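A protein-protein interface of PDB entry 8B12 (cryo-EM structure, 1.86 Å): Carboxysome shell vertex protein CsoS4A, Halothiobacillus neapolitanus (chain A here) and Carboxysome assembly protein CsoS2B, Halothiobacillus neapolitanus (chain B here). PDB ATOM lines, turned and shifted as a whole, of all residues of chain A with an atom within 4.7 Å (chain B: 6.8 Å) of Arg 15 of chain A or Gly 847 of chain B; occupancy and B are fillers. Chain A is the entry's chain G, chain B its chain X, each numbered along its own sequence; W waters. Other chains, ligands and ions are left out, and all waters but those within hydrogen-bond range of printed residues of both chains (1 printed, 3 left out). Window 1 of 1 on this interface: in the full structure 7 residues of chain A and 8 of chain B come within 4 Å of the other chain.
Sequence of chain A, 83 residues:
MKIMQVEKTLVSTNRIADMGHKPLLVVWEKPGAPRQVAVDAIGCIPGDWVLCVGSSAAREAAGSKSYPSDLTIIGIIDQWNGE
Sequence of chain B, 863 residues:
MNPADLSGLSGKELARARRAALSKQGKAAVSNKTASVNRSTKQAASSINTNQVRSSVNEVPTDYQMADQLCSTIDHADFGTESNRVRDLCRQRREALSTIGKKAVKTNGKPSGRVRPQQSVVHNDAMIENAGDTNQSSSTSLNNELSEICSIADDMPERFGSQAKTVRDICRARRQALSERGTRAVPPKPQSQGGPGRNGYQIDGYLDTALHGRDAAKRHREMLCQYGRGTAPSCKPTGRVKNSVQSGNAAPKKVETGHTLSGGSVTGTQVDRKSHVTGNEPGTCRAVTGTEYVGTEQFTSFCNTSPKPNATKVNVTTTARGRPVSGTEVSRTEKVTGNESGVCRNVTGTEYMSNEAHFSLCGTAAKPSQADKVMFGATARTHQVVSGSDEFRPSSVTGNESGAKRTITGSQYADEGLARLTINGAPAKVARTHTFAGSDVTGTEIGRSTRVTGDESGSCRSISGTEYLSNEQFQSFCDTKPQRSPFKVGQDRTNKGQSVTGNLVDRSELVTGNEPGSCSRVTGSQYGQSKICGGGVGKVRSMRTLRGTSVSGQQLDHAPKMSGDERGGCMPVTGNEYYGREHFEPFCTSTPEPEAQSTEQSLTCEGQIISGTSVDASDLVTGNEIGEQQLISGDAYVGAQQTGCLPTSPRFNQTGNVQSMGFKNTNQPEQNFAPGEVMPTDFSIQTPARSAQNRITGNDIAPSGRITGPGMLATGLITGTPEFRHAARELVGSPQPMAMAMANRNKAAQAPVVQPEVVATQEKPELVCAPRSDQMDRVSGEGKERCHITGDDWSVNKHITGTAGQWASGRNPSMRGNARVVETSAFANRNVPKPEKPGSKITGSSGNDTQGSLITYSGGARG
NE2 of His 21 of chain A sits at hydrogen-bond distance from OD2 of Asp 849 of chain B (3.3 Å). The side-chain hydroxyl (OG) of Ser 845 of chain B sits at hydrogen-bond distance from the backbone carbonyl oxygen (O) of Asn 14 of chain A. The backbone carbonyl oxygen (O) of Arg 15 of chain A sits at hydrogen-bond distance from the backbone NH (N) of Gly 847 of chain B, at 2.8 Å. The backbone carbonyl oxygen (O) of Thr 13 of chain A lies close to the backbone carbonyl oxygen (O) of Ser 846 of chain B, 3.4 Å away. The backbone carbonyl oxygen (O) of Thr 13 of chain A is in hydrogen-bond range of the backbone NH (N) of Gly 847 of chain B, 3.5 Å away.
The backbone carbonyl oxygen of Gly 20 of chain A lies within hydrogen-bond range of the guanidinium group of Arg 15 of chain A, at 2.7 Å. The guanidinium group (NH2) of Arg 15 of chain A is in hydrogen-bond range of the backbone carbonyl oxygen (O) of Lys 22 of chain A (2.8 Å). The side-chain hydroxyl (OG) of Ser 12 of chain A is in hydrogen-bond range of the side-chain amide oxygen (OD1) of Asn 14 of chain A (3.5 Å).
Among the printed residues, pairs that only touch across the chains: Ala 17 of chain A with Asn 848 of chain B (3.3 Å), Arg 15 of chain A with Ser 845 of chain B (3.6 Å), Ala 17 of chain A with Asp 849 of chain B (3.6 Å), Gly 20 of chain A with Asp 849 of chain B (3.7 Å), Ile 16 of chain A with Ser 845 of chain B (3.8 Å), Asn 14 of chain A with Ser 846 of chain B (3.95 Å) and Arg 15 of chain A with Ser 846 of chain B (3.98 Å).
Printed residues of chain B within 4 Å of Arg 15 of chain A: Ser 845 (3.6 Å), Ser 846 (3.98 Å) and Gly 847 (2.8 Å). Gly 847 of chain B touches just these residues of chain A: Thr 13 and Arg 15. Printed residues of chain B within 4 Å of Asn 14 of chain A: Ser 845 and Ser 846. Of the printed residues of chain A, Asn 848 of chain B touches Ala 17 (3.3 Å). Of the printed residues of chain B, Gly 20 of chain A touches Asp 849 (3.7 Å). Printed residues of chain B within 4 Å of His 21 of chain A: Asp 849 (3.3 Å). Met 19 of chain A touches none of the printed residues of chain B. Gly 863 of chain B touches none of the printed residues of chain A. The nearest printed residue of chain A that does not touch Asp 849 of chain B is Met 19 of chain A (5.6 Å).
Hydrophobic or aromatic side chains of chain A within 4 Å of the printed part of chain B: Ala 17 and His 21. Of the 8 printed residues of chain B, 5 touch a printed residue of chain A. Printed residues of chain B that touch a printed residue of chain A: Ser 845, Ser 846, Gly 847, Asn 848 and Asp 849. Among the printed residues, no Asp or Glu carboxylate lies within 4 Å of a Lys or Arg side-chain nitrogen of the other chain.
Water W1 lies within hydrogen-bond range of N of Ala 17 of chain A and OG of Ser 845 of chain B.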
ATOM      1  N   SER A  12      12.580   4.941   1.767  1.00  0.00           N
ATOM      2  CA  SER A  12      13.881   5.506   1.411  1.00  0.00           C
ATOM      3  C   SER A  12      14.375   4.772   0.167  1.00  0.00           C
ATOM      4  O   SER A  12      14.932   3.677   0.269  1.00  0.00           O
ATOM      5  CB  SER A  12      14.872   5.387   2.561  1.00  0.00           C
ATOM      6  OG  SER A  12      16.123   5.953   2.221  1.00  0.00           O
ATOM      7  N   THR A  13      14.169   5.383  -1.002  1.00  0.00           N
ATOM      8  CA  THR A  13      14.528   4.730  -2.259  1.00  0.00           C
ATOM      9  C   THR A  13      16.033   4.508  -2.364  1.00  0.00           C
ATOM     10  O   THR A  13      16.481   3.457  -2.832  1.00  0.00           O
ATOM     11  CB  THR A  13      14.026   5.555  -3.445  1.00  0.00           C
ATOM     12  OG1 THR A  13      12.618   5.781  -3.313  1.00  0.00           O
ATOM     13  CG2 THR A  13      14.293   4.825  -4.753  1.00  0.00           C
ATOM     14  N   ASN A  14      16.829   5.484  -1.933  1.00  0.00           N
ATOM     15  CA  ASN A  14      18.275   5.427  -2.082  1.00  0.00           C
ATOM     16  C   ASN A  14      18.973   4.744  -0.906  1.00  0.00           C
ATOM     17  O   ASN A  14      20.189   4.903  -0.749  1.00  0.00           O
ATOM     18  CB  ASN A  14      18.839   6.835  -2.287  1.00  0.00           C
ATOM     19  CG  ASN A  14      18.962   7.608  -0.992  1.00  0.00           C
ATOM     20  OD1 ASN A  14      18.078   7.561  -0.140  1.00  0.00           O
ATOM     21  ND2 ASN A  14      20.068   8.320  -0.835  1.00  0.00           N
ATOM     22  N   ARG A  15      18.244   3.980  -0.096  1.00  0.00           N
ATOM     23  CA  ARG A  15      18.847   3.309   1.047  1.00  0.00           C
ATOM     24  C   ARG A  15      19.868   2.270   0.586  1.00  0.00           C
ATOM     25  O   ARG A  15      19.899   1.864  -0.577  1.00  0.00           O
ATOM     26  CB  ARG A  15      17.773   2.648   1.908  1.00  0.00           C
ATOM     27  CG  ARG A  15      17.321   1.294   1.399  1.00  0.00           C
ATOM     28  CD  ARG A  15      15.909   0.981   1.837  1.00  0.00           C
ATOM     29  NE  ARG A  15      15.654  -0.453   1.840  1.00  0.00           N
ATOM     30  CZ  ARG A  15      14.576  -1.022   2.356  1.00  0.00           C
ATOM     31  NH1 ARG A  15      13.616  -0.305   2.918  1.00  0.00           N
ATOM     32  NH2 ARG A  15      14.457  -2.345   2.312  1.00  0.00           N
ATOM     33  N   ILE A  16      20.720   1.845   1.519  1.00  0.00           N
ATOM     34  CA  ILE A  16      21.801   0.928   1.177  1.00  0.00           C
ATOM     35  C   ILE A  16      21.236  -0.429   0.773  1.00  0.00           C
ATOM     36  O   ILE A  16      20.167  -0.853   1.229  1.00  0.00           O
ATOM     37  CB  ILE A  16      22.795   0.793   2.345  1.00  0.00           C
ATOM     38  CG1 ILE A  16      22.103   0.231   3.591  1.00  0.00           C
ATOM     39  CG2 ILE A  16      23.445   2.131   2.644  1.00  0.00           C
ATOM     40  CD1 ILE A  16      23.054  -0.132   4.706  1.00  0.00           C
ATOM     41  N   ALA A  17      21.971  -1.121  -0.101  1.00  0.00           N
ATOM     42  CA  ALA A  17      21.529  -2.413  -0.611  1.00  0.00           C
ATOM     43  C   ALA A  17      21.443  -3.479   0.474  1.00  0.00           C
ATOM     44  O   ALA A  17      20.709  -4.456   0.304  1.00  0.00           O
ATOM     45  CB  ALA A  17      22.464  -2.883  -1.724  1.00  0.00           C
ATOM     46  N   MET A  19      19.952  -3.353   3.205  1.00  0.00           N
ATOM     47  CA  MET A  19      18.649  -3.366   3.856  1.00  0.00           C
ATOM     48  C   MET A  19      17.694  -4.365   3.216  1.00  0.00           C
ATOM     49  O   MET A  19      16.667  -4.692   3.818  1.00  0.00           O
ATOM     50  CB  MET A  19      18.038  -1.965   3.824  1.00  0.00           C
ATOM     51  CG  MET A  19      18.605  -1.025   4.867  1.00  0.00           C
ATOM     52  SD  MET A  19      17.452   0.260   5.364  1.00  0.00           S
ATOM     53  CE  MET A  19      17.028  -0.312   7.005  1.00  0.00           C
ATOM     54  N   GLY A  20      18.008  -4.859   2.021  1.00  0.00           N
ATOM     55  CA  GLY A  20      17.120  -5.794   1.365  1.00  0.00           C
ATOM     56  C   GLY A  20      15.802  -5.146   0.974  1.00  0.00           C
ATOM     57  O   GLY A  20      15.734  -3.971   0.608  1.00  0.00           O
ATOM     58  N   HIS A  21      14.735  -5.934   1.058  1.00  0.00           N
ATOM     59  CA  HIS A  21      13.397  -5.480   0.712  1.00  0.00           C
ATOM     60  C   HIS A  21      12.526  -5.233   1.936  1.00  0.00           C
ATOM     61  O   HIS A  21      11.310  -5.074   1.793  1.00  0.00           O
ATOM     62  CB  HIS A  21      12.728  -6.496  -0.214  1.00  0.00           C
ATOM     63  CG  HIS A  21      13.442  -6.688  -1.515  1.00  0.00           C
ATOM     64  ND1 HIS A  21      13.363  -7.856  -2.243  1.00  0.00           N
ATOM     65  CD2 HIS A  21      14.252  -5.862  -2.218  1.00  0.00           C
ATOM     66  CE1 HIS A  21      14.091  -7.740  -3.337  1.00  0.00           C
ATOM     67  NE2 HIS A  21      14.640  -6.540  -3.347  1.00  0.00           N
ATOM     68  N   LYS A  22      13.115  -5.199   3.129  1.00  0.00           N
ATOM     69  CA  LYS A  22      12.333  -5.062   4.350  1.00  0.00           C
ATOM     70  C   LYS A  22      11.676  -3.685   4.421  1.00  0.00           C
ATOM     71  O   LYS A  22      12.324  -2.672   4.145  1.00  0.00           O
ATOM     72  CB  LYS A  22      13.212  -5.274   5.583  1.00  0.00           C
ATOM     73  CG  LYS A  22      13.786  -6.669   5.719  1.00  0.00           C
ATOM     74  CD  LYS A  22      12.696  -7.699   5.947  1.00  0.00           C
ATOM     75  CE  LYS A  22      13.153  -8.777   6.914  1.00  0.00           C
ATOM     76  NZ  LYS A  22      12.251  -9.957   6.936  1.00  0.00           N
ATOM     77  N   LEU A  24       9.948  -0.352   6.330  1.00  0.00           N
ATOM     78  CA  LEU A  24      10.273   0.450   7.499  1.00  0.00           C
ATOM     79  C   LEU A  24       9.032   1.185   7.982  1.00  0.00           C
ATOM     80  O   LEU A  24       8.263   1.719   7.179  1.00  0.00           O
ATOM     81  CB  LEU A  24      11.387   1.452   7.190  1.00  0.00           C
ATOM     82  CG  LEU A  24      12.628   0.876   6.507  1.00  0.00           C
ATOM     83  CD1 LEU A  24      13.548   1.984   6.040  1.00  0.00           C
ATOM     84  CD2 LEU A  24      13.354  -0.073   7.441  1.00  0.00           C
ATOM     85  N   GLY B 844      25.776   3.693  -7.346  1.00  0.00           N
ATOM     86  CA  GLY B 844      25.130   4.632  -6.456  1.00  0.00           C
ATOM     87  C   GLY B 844      24.126   3.942  -5.549  1.00  0.00           C
ATOM     88  O   GLY B 844      23.679   2.824  -5.799  1.00  0.00           O
ATOM     89  N   SER B 845      23.770   4.628  -4.470  1.00  0.00           N
ATOM     90  CA  SER B 845      22.875   4.052  -3.472  1.00  0.00           C
ATOM     91  C   SER B 845      21.442   4.136  -3.987  1.00  0.00           C
ATOM     92  O   SER B 845      20.869   5.226  -4.077  1.00  0.00           O
ATOM     93  CB  SER B 845      23.032   4.765  -2.134  1.00  0.00           C
ATOM     94  OG  SER B 845      22.858   3.855  -1.064  1.00  0.00           O
ATOM     95  N   SER B 846      20.871   2.987  -4.349  1.00  0.00           N
ATOM     96  CA  SER B 846      19.518   2.939  -4.890  1.00  0.00           C
ATOM     97  C   SER B 846      18.753   1.718  -4.389  1.00  0.00           C
ATOM     98  O   SER B 846      17.850   1.229  -5.074  1.00  0.00           O
ATOM     99  CB  SER B 846      19.541   2.940  -6.420  1.00  0.00           C
ATOM    100  OG  SER B 846      20.385   1.913  -6.906  1.00  0.00           O
ATOM    101  N   GLY B 847      19.101   1.213  -3.209  1.00  0.00           N
ATOM    102  CA  GLY B 847      18.472   0.003  -2.698  1.00  0.00           C
ATOM    103  C   GLY B 847      18.677  -1.201  -3.591  1.00  0.00           C
ATOM    104  O   GLY B 847      17.750  -1.999  -3.779  1.00  0.00           O
ATOM    105  N   ASN B 848      19.882  -1.356  -4.141  1.00  0.00           N
ATOM    106  CA  ASN B 848      20.157  -2.365  -5.166  1.00  0.00           C
ATOM    107  C   ASN B 848      20.493  -3.704  -4.506  1.00  0.00           C
ATOM    108  O   ASN B 848      21.608  -4.222  -4.585  1.00  0.00           O
ATOM    109  CB  ASN B 848      21.279  -1.894  -6.078  1.00  0.00           C
ATOM    110  CG  ASN B 848      21.277  -2.596  -7.419  1.00  0.00           C
ATOM    111  OD1 ASN B 848      20.222  -2.868  -7.988  1.00  0.00           O
ATOM    112  ND2 ASN B 848      22.462  -2.901  -7.929  1.00  0.00           N
ATOM    113  N   ASP B 849      19.487  -4.275  -3.849  1.00  0.00           N
ATOM    114  CA  ASP B 849      19.646  -5.587  -3.237  1.00  0.00           C
ATOM    115  C   ASP B 849      19.672  -6.660  -4.319  1.00  0.00           C
ATOM    116  O   ASP B 849      18.837  -6.660  -5.227  1.00  0.00           O
ATOM    117  CB  ASP B 849      18.516  -5.846  -2.241  1.00  0.00           C
ATOM    118  CG  ASP B 849      18.314  -7.321  -1.958  1.00  0.00           C
ATOM    119  OD1 ASP B 849      18.969  -7.844  -1.034  1.00  0.00           O
ATOM    120  OD2 ASP B 849      17.498  -7.956  -2.656  1.00  0.00           O
ATOM    121  N   THR B 850      20.639  -7.570  -4.228  1.00  0.00           N
ATOM    122  CA  THR B 850      20.819  -8.612  -5.230  1.00  0.00           C
ATOM    123  C   THR B 850      20.492 -10.007  -4.718  1.00  0.00           C
ATOM    124  O   THR B 850      20.623 -10.974  -5.475  1.00  0.00           O
ATOM    125  CB  THR B 850      22.255  -8.599  -5.765  1.00  0.00           C
ATOM    126  OG1 THR B 850      23.148  -9.106  -4.764  1.00  0.00           O
ATOM    127  CG2 THR B 850      22.676  -7.188  -6.144  1.00  0.00           C
ATOM    128  N   GLY B 863      15.110  -4.605 -10.761  1.00  0.00           N
ATOM    129  CA  GLY B 863      14.793  -3.531  -9.839  1.00  0.00           C
ATOM    130  C   GLY B 863      14.346  -4.002  -8.471  1.00  0.00           C
ATOM    131  O   GLY B 863      15.168  -4.310  -7.608  1.00  0.00           O
HETATM  132  O   HOH W   1      23.861   0.577  -1.384  1.00  0.00           O
